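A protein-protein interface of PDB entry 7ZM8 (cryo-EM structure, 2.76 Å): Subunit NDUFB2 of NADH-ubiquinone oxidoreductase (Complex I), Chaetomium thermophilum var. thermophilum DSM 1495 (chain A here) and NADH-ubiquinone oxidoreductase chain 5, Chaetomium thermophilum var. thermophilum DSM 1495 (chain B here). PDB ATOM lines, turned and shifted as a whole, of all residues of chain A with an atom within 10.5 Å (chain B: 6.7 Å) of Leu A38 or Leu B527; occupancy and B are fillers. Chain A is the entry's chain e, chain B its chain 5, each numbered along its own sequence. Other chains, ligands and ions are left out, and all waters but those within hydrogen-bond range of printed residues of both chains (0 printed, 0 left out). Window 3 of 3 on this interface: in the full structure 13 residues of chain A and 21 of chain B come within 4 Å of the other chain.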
ATOM      1  N   ILE A  27       6.360  -4.916  30.881  1.00  0.00           N
ATOM      2  CA  ILE A  27       7.399  -5.517  29.997  1.00  0.00           C
ATOM      3  C   ILE A  27       6.728  -6.136  28.765  1.00  0.00           C
ATOM      4  O   ILE A  27       7.120  -5.755  27.650  1.00  0.00           O
ATOM      5  CB  ILE A  27       8.280  -6.520  30.768  1.00  0.00           C
ATOM      6  CG1 ILE A  27       9.034  -5.836  31.911  1.00  0.00           C
ATOM      7  CG2 ILE A  27       9.231  -7.242  29.827  1.00  0.00           C
ATOM      8  CD1 ILE A  27       9.856  -4.648  31.476  1.00  0.00           C
ATOM      9  N   ARG A  30       4.780  -3.574  26.658  1.00  0.00           N
ATOM     10  CA  ARG A  30       5.691  -2.794  25.837  1.00  0.00           C
ATOM     11  C   ARG A  30       6.293  -3.633  24.724  1.00  0.00           C
ATOM     12  O   ARG A  30       6.605  -3.108  23.652  1.00  0.00           O
ATOM     13  CB  ARG A  30       6.789  -2.192  26.707  1.00  0.00           C
ATOM     14  CG  ARG A  30       6.321  -1.080  27.616  1.00  0.00           C
ATOM     15  CD  ARG A  30       6.583   0.272  27.000  1.00  0.00           C
ATOM     16  NE  ARG A  30       6.018   0.386  25.662  1.00  0.00           N
ATOM     17  CZ  ARG A  30       4.724   0.525  25.404  1.00  0.00           C
ATOM     18  NH1 ARG A  30       3.849   0.574  26.395  1.00  0.00           N
ATOM     19  NH2 ARG A  30       4.305   0.619  24.152  1.00  0.00           N
ATOM     20  N   ALA A  31       6.477  -4.931  24.963  1.00  0.00           N
ATOM     21  CA  ALA A  31       6.957  -5.813  23.909  1.00  0.00           C
ATOM     22  C   ALA A  31       5.873  -6.069  22.875  1.00  0.00           C
ATOM     23  O   ALA A  31       6.147  -6.094  21.674  1.00  0.00           O
ATOM     24  CB  ALA A  31       7.449  -7.128  24.511  1.00  0.00           C
ATOM     25  N   LYS A  32       4.634  -6.259  23.319  1.00  0.00           N
ATOM     26  CA  LYS A  32       3.551  -6.472  22.369  1.00  0.00           C
ATOM     27  C   LYS A  32       3.328  -5.242  21.502  1.00  0.00           C
ATOM     28  O   LYS A  32       2.970  -5.370  20.326  1.00  0.00           O
ATOM     29  CB  LYS A  32       2.270  -6.851  23.111  1.00  0.00           C
ATOM     30  CG  LYS A  32       1.019  -6.837  22.252  1.00  0.00           C
ATOM     31  CD  LYS A  32      -0.112  -7.606  22.908  1.00  0.00           C
ATOM     32  CE  LYS A  32      -1.449  -7.260  22.276  1.00  0.00           C
ATOM     33  NZ  LYS A  32      -1.808  -5.832  22.491  1.00  0.00           N
ATOM     34  N   LYS A  33       3.554  -4.050  22.049  1.00  0.00           N
ATOM     35  CA  LYS A  33       3.304  -2.824  21.308  1.00  0.00           C
ATOM     36  C   LYS A  33       4.534  -2.328  20.563  1.00  0.00           C
ATOM     37  O   LYS A  33       4.425  -1.902  19.410  1.00  0.00           O
ATOM     38  CB  LYS A  33       2.795  -1.737  22.255  1.00  0.00           C
ATOM     39  CG  LYS A  33       2.056  -0.608  21.562  1.00  0.00           C
ATOM     40  CD  LYS A  33       1.141   0.126  22.527  1.00  0.00           C
ATOM     41  CE  LYS A  33       0.922   1.568  22.094  1.00  0.00           C
ATOM     42  NZ  LYS A  33       2.165   2.376  22.212  1.00  0.00           N
ATOM     43  N   ASP A  34       5.707  -2.375  21.190  1.00  0.00           N
ATOM     44  CA  ASP A  34       6.915  -1.824  20.594  1.00  0.00           C
ATOM     45  C   ASP A  34       7.928  -2.882  20.187  1.00  0.00           C
ATOM     46  O   ASP A  34       9.005  -2.529  19.696  1.00  0.00           O
ATOM     47  CB  ASP A  34       7.573  -0.830  21.558  1.00  0.00           C
ATOM     48  CG  ASP A  34       6.754   0.433  21.735  1.00  0.00           C
ATOM     49  OD1 ASP A  34       6.033   0.812  20.789  1.00  0.00           O
ATOM     50  OD2 ASP A  34       6.829   1.045  22.821  1.00  0.00           O
ATOM     51  N   GLY A  35       7.622  -4.157  20.383  1.00  0.00           N
ATOM     52  CA  GLY A  35       8.508  -5.228  20.000  1.00  0.00           C
ATOM     53  C   GLY A  35       8.768  -5.329  18.512  1.00  0.00           C
ATOM     54  O   GLY A  35       9.921  -5.309  18.076  1.00  0.00           O
ATOM     55  N   PRO A  36       7.714  -5.447  17.697  1.00  0.00           N
ATOM     56  CA  PRO A  36       7.943  -5.603  16.252  1.00  0.00           C
ATOM     57  C   PRO A  36       8.712  -4.455  15.635  1.00  0.00           C
ATOM     58  O   PRO A  36       9.508  -4.683  14.718  1.00  0.00           O
ATOM     59  CB  PRO A  36       6.526  -5.714  15.669  1.00  0.00           C
ATOM     60  CG  PRO A  36       5.614  -5.218  16.707  1.00  0.00           C
ATOM     61  CD  PRO A  36       6.280  -5.397  18.030  1.00  0.00           C
ATOM     62  N   VAL A  37       8.528  -3.248  16.161  1.00  0.00           N
ATOM     63  CA  VAL A  37       9.256  -2.058  15.639  1.00  0.00           C
ATOM     64  C   VAL A  37      10.707  -2.170  16.090  1.00  0.00           C
ATOM     65  O   VAL A  37      11.596  -1.840  15.289  1.00  0.00           O
ATOM     66  CB  VAL A  37       8.627  -0.742  16.126  1.00  0.00           C
ATOM     67  CG1 VAL A  37       9.202   0.461  15.396  1.00  0.00           C
ATOM     68  CG2 VAL A  37       7.112  -0.766  16.004  1.00  0.00           C
ATOM     69  N   LEU A  38      10.930  -2.645  17.315  1.00  0.00           N
ATOM     70  CA  LEU A  38      12.277  -2.732  17.863  1.00  0.00           C
ATOM     71  C   LEU A  38      13.105  -3.786  17.142  1.00  0.00           C
ATOM     72  O   LEU A  38      14.278  -3.555  16.833  1.00  0.00           O
ATOM     73  CB  LEU A  38      12.213  -3.030  19.359  1.00  0.00           C
ATOM     74  CG  LEU A  38      13.484  -2.789  20.177  1.00  0.00           C
ATOM     75  CD1 LEU A  38      13.126  -2.255  21.551  1.00  0.00           C
ATOM     76  CD2 LEU A  38      14.305  -4.063  20.303  1.00  0.00           C
ATOM     77  N   LEU A  39      12.514  -4.940  16.855  1.00  0.00           N
ATOM     78  CA  LEU A  39      13.254  -6.039  16.252  1.00  0.00           C
ATOM     79  C   LEU A  39      13.192  -6.044  14.731  1.00  0.00           C
ATOM     80  O   LEU A  39      13.563  -7.047  14.115  1.00  0.00           O
ATOM     81  CB  LEU A  39      12.769  -7.377  16.830  1.00  0.00           C
ATOM     82  CG  LEU A  39      11.309  -7.822  16.721  1.00  0.00           C
ATOM     83  CD1 LEU A  39      11.019  -8.548  15.425  1.00  0.00           C
ATOM     84  CD2 LEU A  39      10.936  -8.686  17.917  1.00  0.00           C
ATOM     85  N   GLY A  40      12.746  -4.954  14.113  1.00  0.00           N
ATOM     86  CA  GLY A  40      12.976  -4.698  12.702  1.00  0.00           C
ATOM     87  C   GLY A  40      11.840  -5.078  11.777  1.00  0.00           C
ATOM     88  O   GLY A  40      11.909  -4.772  10.578  1.00  0.00           O
ATOM     89  N   TRP A  41      10.841  -5.783  12.304  1.00  0.00           N
ATOM     90  CA  TRP A  41       9.736  -6.273  11.441  1.00  0.00           C
ATOM     91  C   TRP A  41       8.848  -5.110  10.992  1.00  0.00           C
ATOM     92  O   TRP A  41       8.180  -5.255   9.952  1.00  0.00           O
ATOM     93  CB  TRP A  41       8.934  -7.353  12.174  1.00  0.00           C
ATOM     94  CG  TRP A  41       9.335  -8.748  11.806  1.00  0.00           C
ATOM     95  CD1 TRP A  41      10.508  -9.375  12.110  1.00  0.00           C
ATOM     96  CD2 TRP A  41       8.558  -9.697  11.056  1.00  0.00           C
ATOM     97  NE1 TRP A  41      10.514 -10.645  11.602  1.00  0.00           N
ATOM     98  CE2 TRP A  41       9.332 -10.872  10.950  1.00  0.00           C
ATOM     99  CE3 TRP A  41       7.290  -9.670  10.465  1.00  0.00           C
ATOM    100  CZ2 TRP A  41       8.875 -12.006  10.280  1.00  0.00           C
ATOM    101  CZ3 TRP A  41       6.840 -10.790   9.802  1.00  0.00           C
ATOM    102  CH2 TRP A  41       7.624 -11.941   9.712  1.00  0.00           C
ATOM    103  N   LYS A  42       8.918  -3.981  11.701  1.00  0.00           N
ATOM    104  CA  LYS A  42       8.004  -2.848  11.397  1.00  0.00           C
ATOM    105  C   LYS A  42       8.791  -1.549  11.214  1.00  0.00           C
ATOM    106  O   LYS A  42      10.032  -1.599  11.263  1.00  0.00           O
ATOM    107  CB  LYS A  42       6.945  -2.703  12.493  1.00  0.00           C
ATOM    108  CG  LYS A  42       5.830  -3.740  12.467  1.00  0.00           C
ATOM    109  CD  LYS A  42       4.942  -3.628  11.247  1.00  0.00           C
ATOM    110  CE  LYS A  42       4.209  -2.305  11.169  1.00  0.00           C
ATOM    111  NZ  LYS A  42       3.360  -2.077  12.362  1.00  0.00           N
ATOM    112  N   HIS A  43       8.206  -0.453  11.136  1.00  0.00           N
ATOM    113  CA  HIS A  43       8.866   0.873  11.064  1.00  0.00           C
ATOM    114  C   HIS A  43       7.953   1.809  11.880  1.00  0.00           C
ATOM    115  O   HIS A  43       6.743   1.518  11.891  1.00  0.00           O
ATOM    116  CB  HIS A  43       8.953   1.354   9.611  1.00  0.00           C
ATOM    117  CG  HIS A  43      10.341   1.400   9.073  1.00  0.00           C
ATOM    118  ND1 HIS A  43      10.648   0.992   7.791  1.00  0.00           N
ATOM    119  CD2 HIS A  43      11.503   1.796   9.634  1.00  0.00           C
ATOM    120  CE1 HIS A  43      11.940   1.140   7.583  1.00  0.00           C
ATOM    121  NE2 HIS A  43      12.487   1.633   8.698  1.00  0.00           N
ATOM    122  N   PRO A  44       8.327   2.896  12.466  1.00  0.00           N
ATOM    123  CA  PRO A  44       7.443   3.688  13.315  1.00  0.00           C
ATOM    124  C   PRO A  44       6.563   4.590  12.444  1.00  0.00           C
ATOM    125  O   PRO A  44       6.598   5.784  12.661  1.00  0.00           O
ATOM    126  CB  PRO A  44       8.408   4.571  14.123  1.00  0.00           C
ATOM    127  CG  PRO A  44       9.793   4.005  13.861  1.00  0.00           C
ATOM    128  CD  PRO A  44       9.718   3.329  12.508  1.00  0.00           C
ATOM    129  N   TRP A  45       5.778   3.998  11.534  1.00  0.00           N
ATOM    130  CA  TRP A  45       4.884   4.758  10.618  1.00  0.00           C
ATOM    131  C   TRP A  45       4.131   3.767   9.725  1.00  0.00           C
ATOM    132  O   TRP A  45       4.604   2.619   9.629  1.00  0.00           O
ATOM    133  CB  TRP A  45       5.646   5.800   9.784  1.00  0.00           C
ATOM    134  CG  TRP A  45       6.790   5.279   8.971  1.00  0.00           C
ATOM    135  CD1 TRP A  45       6.726   4.608   7.785  1.00  0.00           C
ATOM    136  CD2 TRP A  45       8.190   5.438   9.262  1.00  0.00           C
ATOM    137  NE1 TRP A  45       7.983   4.319   7.332  1.00  0.00           N
ATOM    138  CE2 TRP A  45       8.902   4.818   8.216  1.00  0.00           C
ATOM    139  CE3 TRP A  45       8.906   6.037  10.303  1.00  0.00           C
ATOM    140  CZ2 TRP A  45      10.293   4.780   8.188  1.00  0.00           C
ATOM    141  CZ3 TRP A  45      10.280   5.995  10.276  1.00  0.00           C
ATOM    142  CH2 TRP A  45      10.962   5.371   9.234  1.00  0.00           C
ATOM    143  N   PRO B 384      15.101  -4.596  28.427  1.00  0.00           N
ATOM    144  CA  PRO B 384      14.177  -3.870  27.553  1.00  0.00           C
ATOM    145  C   PRO B 384      12.975  -3.314  28.301  1.00  0.00           C
ATOM    146  O   PRO B 384      12.411  -3.962  29.183  1.00  0.00           O
ATOM    147  CB  PRO B 384      13.752  -4.932  26.537  1.00  0.00           C
ATOM    148  CG  PRO B 384      14.801  -6.013  26.611  1.00  0.00           C
ATOM    149  CD  PRO B 384      15.761  -5.696  27.713  1.00  0.00           C
ATOM    150  N   PHE B 385      12.616  -2.079  27.948  1.00  0.00           N
ATOM    151  CA  PHE B 385      11.421  -1.382  28.407  1.00  0.00           C
ATOM    152  C   PHE B 385      11.491  -0.974  29.872  1.00  0.00           C
ATOM    153  O   PHE B 385      10.470  -0.636  30.470  1.00  0.00           O
ATOM    154  CB  PHE B 385      10.164  -2.212  28.138  1.00  0.00           C
ATOM    155  CG  PHE B 385      10.103  -2.771  26.749  1.00  0.00           C
ATOM    156  CD1 PHE B 385      10.083  -1.934  25.653  1.00  0.00           C
ATOM    157  CD2 PHE B 385      10.069  -4.133  26.539  1.00  0.00           C
ATOM    158  CE1 PHE B 385      10.026  -2.447  24.375  1.00  0.00           C
ATOM    159  CE2 PHE B 385      10.017  -4.650  25.267  1.00  0.00           C
ATOM    160  CZ  PHE B 385       9.993  -3.805  24.182  1.00  0.00           C
ATOM    161  N   PHE B 389      16.702   1.285  30.073  1.00  0.00           N
ATOM    162  CA  PHE B 389      16.772   0.797  28.701  1.00  0.00           C
ATOM    163  C   PHE B 389      16.855   1.946  27.708  1.00  0.00           C
ATOM    164  O   PHE B 389      17.640   1.904  26.754  1.00  0.00           O
ATOM    165  CB  PHE B 389      15.559  -0.077  28.413  1.00  0.00           C
ATOM    166  CG  PHE B 389      15.455  -0.519  26.993  1.00  0.00           C
ATOM    167  CD1 PHE B 389      16.419  -1.326  26.436  1.00  0.00           C
ATOM    168  CD2 PHE B 389      14.382  -0.134  26.217  1.00  0.00           C
ATOM    169  CE1 PHE B 389      16.318  -1.736  25.134  1.00  0.00           C
ATOM    170  CE2 PHE B 389      14.276  -0.541  24.917  1.00  0.00           C
ATOM    171  CZ  PHE B 389      15.247  -1.342  24.374  1.00  0.00           C
ATOM    172  N   GLU B 397      24.093   2.780  20.910  1.00  0.00           N
ATOM    173  CA  GLU B 397      23.810   2.883  19.488  1.00  0.00           C
ATOM    174  C   GLU B 397      24.137   4.256  18.919  1.00  0.00           C
ATOM    175  O   GLU B 397      24.278   4.388  17.701  1.00  0.00           O
ATOM    176  CB  GLU B 397      22.352   2.510  19.226  1.00  0.00           C
ATOM    177  CG  GLU B 397      21.327   3.440  19.825  1.00  0.00           C
ATOM    178  CD  GLU B 397      19.911   2.956  19.574  1.00  0.00           C
ATOM    179  OE1 GLU B 397      19.751   1.885  18.952  1.00  0.00           O
ATOM    180  OE2 GLU B 397      18.960   3.637  20.003  1.00  0.00           O
ATOM    181  N   TYR B 411      32.058   1.795  21.279  1.00  0.00           N
ATOM    182  CA  TYR B 411      30.957   0.841  21.284  1.00  0.00           C
ATOM    183  C   TYR B 411      31.430  -0.539  21.716  1.00  0.00           C
ATOM    184  O   TYR B 411      30.771  -1.208  22.519  1.00  0.00           O
ATOM    185  CB  TYR B 411      30.302   0.770  19.908  1.00  0.00           C
ATOM    186  CG  TYR B 411      29.199  -0.260  19.847  1.00  0.00           C
ATOM    187  CD1 TYR B 411      27.910   0.052  20.247  1.00  0.00           C
ATOM    188  CD2 TYR B 411      29.455  -1.553  19.417  1.00  0.00           C
ATOM    189  CE1 TYR B 411      26.908  -0.884  20.201  1.00  0.00           C
ATOM    190  CE2 TYR B 411      28.460  -2.494  19.382  1.00  0.00           C
ATOM    191  CZ  TYR B 411      27.189  -2.153  19.768  1.00  0.00           C
ATOM    192  OH  TYR B 411      26.194  -3.095  19.727  1.00  0.00           O
ATOM    193  N   PRO B 522      22.718  -0.788  12.299  1.00  0.00           N
ATOM    194  CA  PRO B 522      22.038  -2.045  11.987  1.00  0.00           C
ATOM    195  C   PRO B 522      21.319  -2.606  13.200  1.00  0.00           C
ATOM    196  O   PRO B 522      21.617  -2.277  14.349  1.00  0.00           O
ATOM    197  CB  PRO B 522      23.179  -2.965  11.543  1.00  0.00           C
ATOM    198  CG  PRO B 522      24.386  -2.399  12.186  1.00  0.00           C
ATOM    199  CD  PRO B 522      24.182  -0.920  12.233  1.00  0.00           C
ATOM    200  N   VAL B 523      20.342  -3.467  12.919  1.00  0.00           N
ATOM    201  CA  VAL B 523      19.533  -4.044  13.986  1.00  0.00           C
ATOM    202  C   VAL B 523      20.370  -4.954  14.873  1.00  0.00           C
ATOM    203  O   VAL B 523      20.078  -5.109  16.064  1.00  0.00           O
ATOM    204  CB  VAL B 523      18.320  -4.782  13.386  1.00  0.00           C
ATOM    205  CG1 VAL B 523      18.771  -5.957  12.535  1.00  0.00           C
ATOM    206  CG2 VAL B 523      17.365  -5.232  14.480  1.00  0.00           C
ATOM    207  N   LEU B 524      21.418  -5.571  14.323  1.00  0.00           N
ATOM    208  CA  LEU B 524      22.243  -6.472  15.120  1.00  0.00           C
ATOM    209  C   LEU B 524      22.932  -5.727  16.253  1.00  0.00           C
ATOM    210  O   LEU B 524      22.853  -6.134  17.416  1.00  0.00           O
ATOM    211  CB  LEU B 524      23.272  -7.170  14.234  1.00  0.00           C
ATOM    212  CG  LEU B 524      22.874  -8.550  13.712  1.00  0.00           C
ATOM    213  CD1 LEU B 524      21.822  -8.436  12.619  1.00  0.00           C
ATOM    214  CD2 LEU B 524      24.097  -9.302  13.211  1.00  0.00           C
ATOM    215  N   PHE B 525      23.609  -4.626  15.929  1.00  0.00           N
ATOM    216  CA  PHE B 525      24.258  -3.833  16.964  1.00  0.00           C
ATOM    217  C   PHE B 525      23.237  -3.143  17.853  1.00  0.00           C
ATOM    218  O   PHE B 525      23.510  -2.892  19.030  1.00  0.00           O
ATOM    219  CB  PHE B 525      25.194  -2.810  16.328  1.00  0.00           C
ATOM    220  CG  PHE B 525      26.420  -3.415  15.715  1.00  0.00           C
ATOM    221  CD1 PHE B 525      26.345  -4.106  14.519  1.00  0.00           C
ATOM    222  CD2 PHE B 525      27.648  -3.297  16.333  1.00  0.00           C
ATOM    223  CE1 PHE B 525      27.468  -4.663  13.953  1.00  0.00           C
ATOM    224  CE2 PHE B 525      28.778  -3.852  15.772  1.00  0.00           C
ATOM    225  CZ  PHE B 525      28.688  -4.537  14.579  1.00  0.00           C
ATOM    226  N   LYS B 526      22.065  -2.823  17.306  1.00  0.00           N
ATOM    227  CA  LYS B 526      21.003  -2.252  18.122  1.00  0.00           C
ATOM    228  C   LYS B 526      20.516  -3.250  19.162  1.00  0.00           C
ATOM    229  O   LYS B 526      20.231  -2.877  20.305  1.00  0.00           O
ATOM    230  CB  LYS B 526      19.850  -1.796  17.232  1.00  0.00           C
ATOM    231  CG  LYS B 526      20.056  -0.425  16.620  1.00  0.00           C
ATOM    232  CD  LYS B 526      18.880  -0.031  15.749  1.00  0.00           C
ATOM    233  CE  LYS B 526      18.898   1.455  15.436  1.00  0.00           C
ATOM    234  NZ  LYS B 526      17.638   1.894  14.775  1.00  0.00           N
ATOM    235  N   LEU B 527      20.413  -4.518  18.783  1.00  0.00           N
ATOM    236  CA  LEU B 527      19.955  -5.563  19.683  1.00  0.00           C
ATOM    237  C   LEU B 527      21.093  -6.260  20.414  1.00  0.00           C
ATOM    238  O   LEU B 527      20.833  -6.999  21.367  1.00  0.00           O
ATOM    239  CB  LEU B 527      19.141  -6.599  18.902  1.00  0.00           C
ATOM    240  CG  LEU B 527      18.099  -7.395  19.686  1.00  0.00           C
ATOM    241  CD1 LEU B 527      17.172  -6.459  20.442  1.00  0.00           C
ATOM    242  CD2 LEU B 527      17.311  -8.302  18.757  1.00  0.00           C
ATOM    243  N   LEU B 528      22.341  -6.014  20.013  1.00  0.00           N
ATOM    244  CA  LEU B 528      23.464  -6.772  20.561  1.00  0.00           C
ATOM    245  C   LEU B 528      23.578  -6.712  22.080  1.00  0.00           C
ATOM    246  O   LEU B 528      23.801  -7.772  22.687  1.00  0.00           O
ATOM    247  CB  LEU B 528      24.772  -6.306  19.909  1.00  0.00           C
ATOM    248  CG  LEU B 528      25.965  -7.242  20.098  1.00  0.00           C
ATOM    249  CD1 LEU B 528      25.602  -8.662  19.697  1.00  0.00           C
ATOM    250  CD2 LEU B 528      27.163  -6.749  19.306  1.00  0.00           C
ATOM    251  N   PRO B 529      23.455  -5.560  22.749  1.00  0.00           N
ATOM    252  CA  PRO B 529      23.561  -5.576  24.219  1.00  0.00           C
ATOM    253  C   PRO B 529      22.530  -6.459  24.895  1.00  0.00           C
ATOM    254  O   PRO B 529      22.813  -7.001  25.969  1.00  0.00           O
ATOM    255  CB  PRO B 529      23.378  -4.102  24.601  1.00  0.00           C
ATOM    256  CG  PRO B 529      23.789  -3.350  23.396  1.00  0.00           C
ATOM    257  CD  PRO B 529      23.346  -4.183  22.234  1.00  0.00           C
ATOM    258  N   PHE B 530      21.342  -6.620  24.307  1.00  0.00           N
ATOM    259  CA  PHE B 530      20.309  -7.427  24.949  1.00  0.00           C
ATOM    260  C   PHE B 530      20.704  -8.897  25.012  1.00  0.00           C
ATOM    261  O   PHE B 530      20.581  -9.535  26.063  1.00  0.00           O
ATOM    262  CB  PHE B 530      18.976  -7.267  24.220  1.00  0.00           C
ATOM    263  CG  PHE B 530      17.875  -8.114  24.791  1.00  0.00           C
ATOM    264  CD1 PHE B 530      17.699  -8.214  26.161  1.00  0.00           C
ATOM    265  CD2 PHE B 530      17.023  -8.818  23.960  1.00  0.00           C
ATOM    266  CE1 PHE B 530      16.694  -8.998  26.690  1.00  0.00           C
ATOM    267  CE2 PHE B 530      16.015  -9.602  24.483  1.00  0.00           C
ATOM    268  CZ  PHE B 530      15.850  -9.691  25.849  1.00  0.00           C
ATOM    269  N   ILE B 531      21.172  -9.459  23.895  1.00  0.00           N
ATOM    270  CA  ILE B 531      21.557 -10.869  23.890  1.00  0.00           C
ATOM    271  C   ILE B 531      22.690 -11.114  24.874  1.00  0.00           C
ATOM    272  O   ILE B 531      22.717 -12.135  25.571  1.00  0.00           O
ATOM    273  CB  ILE B 531      21.927 -11.339  22.470  1.00  0.00           C
ATOM    274  CG1 ILE B 531      20.717 -11.291  21.534  1.00  0.00           C
ATOM    275  CG2 ILE B 531      22.502 -12.742  22.497  1.00  0.00           C
ATOM    276  CD1 ILE B 531      20.530  -9.995  20.805  1.00  0.00           C
ATOM    277  N   PHE B 532      23.637 -10.179  24.957  1.00  0.00           N
ATOM    278  CA  PHE B 532      24.757 -10.350  25.875  1.00  0.00           C
ATOM    279  C   PHE B 532      24.286 -10.404  27.322  1.00  0.00           C
ATOM    280  O   PHE B 532      24.768 -11.225  28.107  1.00  0.00           O
ATOM    281  CB  PHE B 532      25.773  -9.230  25.675  1.00  0.00           C
ATOM    282  CG  PHE B 532      26.637  -9.412  24.465  1.00  0.00           C
ATOM    283  CD1 PHE B 532      26.879 -10.677  23.960  1.00  0.00           C
ATOM    284  CD2 PHE B 532      27.209  -8.324  23.835  1.00  0.00           C
ATOM    285  CE1 PHE B 532      27.674 -10.854  22.846  1.00  0.00           C
ATOM    286  CE2 PHE B 532      28.006  -8.494  22.722  1.00  0.00           C
ATOM    287  CZ  PHE B 532      28.239  -9.760  22.227  1.00  0.00           C
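Leu B527 touches just one residue of chain A: Leu A38 (3.7 Å).
No residue of chain A comes within 4 Å of Val B523.
Leu B528 touches none of the printed residues of chain A.
No residue of chain A comes within 4 Å of Pro B529.
Printed residues of chain A within 4 Å of Phe B385: Ile A27, Arg A30 and Ala A31.
Of the printed residues of chain A, Phe B389 touches Leu A38 (3.6 Å).
Lys A42 touches none of the printed residues of chain B.
The nearest residue of chain B that does not touch Leu A38 is Phe B385 (4.2 Å).
The nearest residue of chain A that does not touch Leu B527 is Leu A39 (5.0 Å).
Among the printed residues, pairs that only touch across the chains: Arg A30 with Phe B385, Ile A27 with Pro B384, Ala A31 with Phe B385, Ile A27 with Phe B385, Leu A38 with Phe B389 and Leu A38 with Leu B527.
Among the printed residues, 6 pairs touch across the chains.
The guanidinium group (NH2) of Arg A30 is in salt-bridge range of the side-chain carboxylate (OD2) of Asp A34 (2.9 Å).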
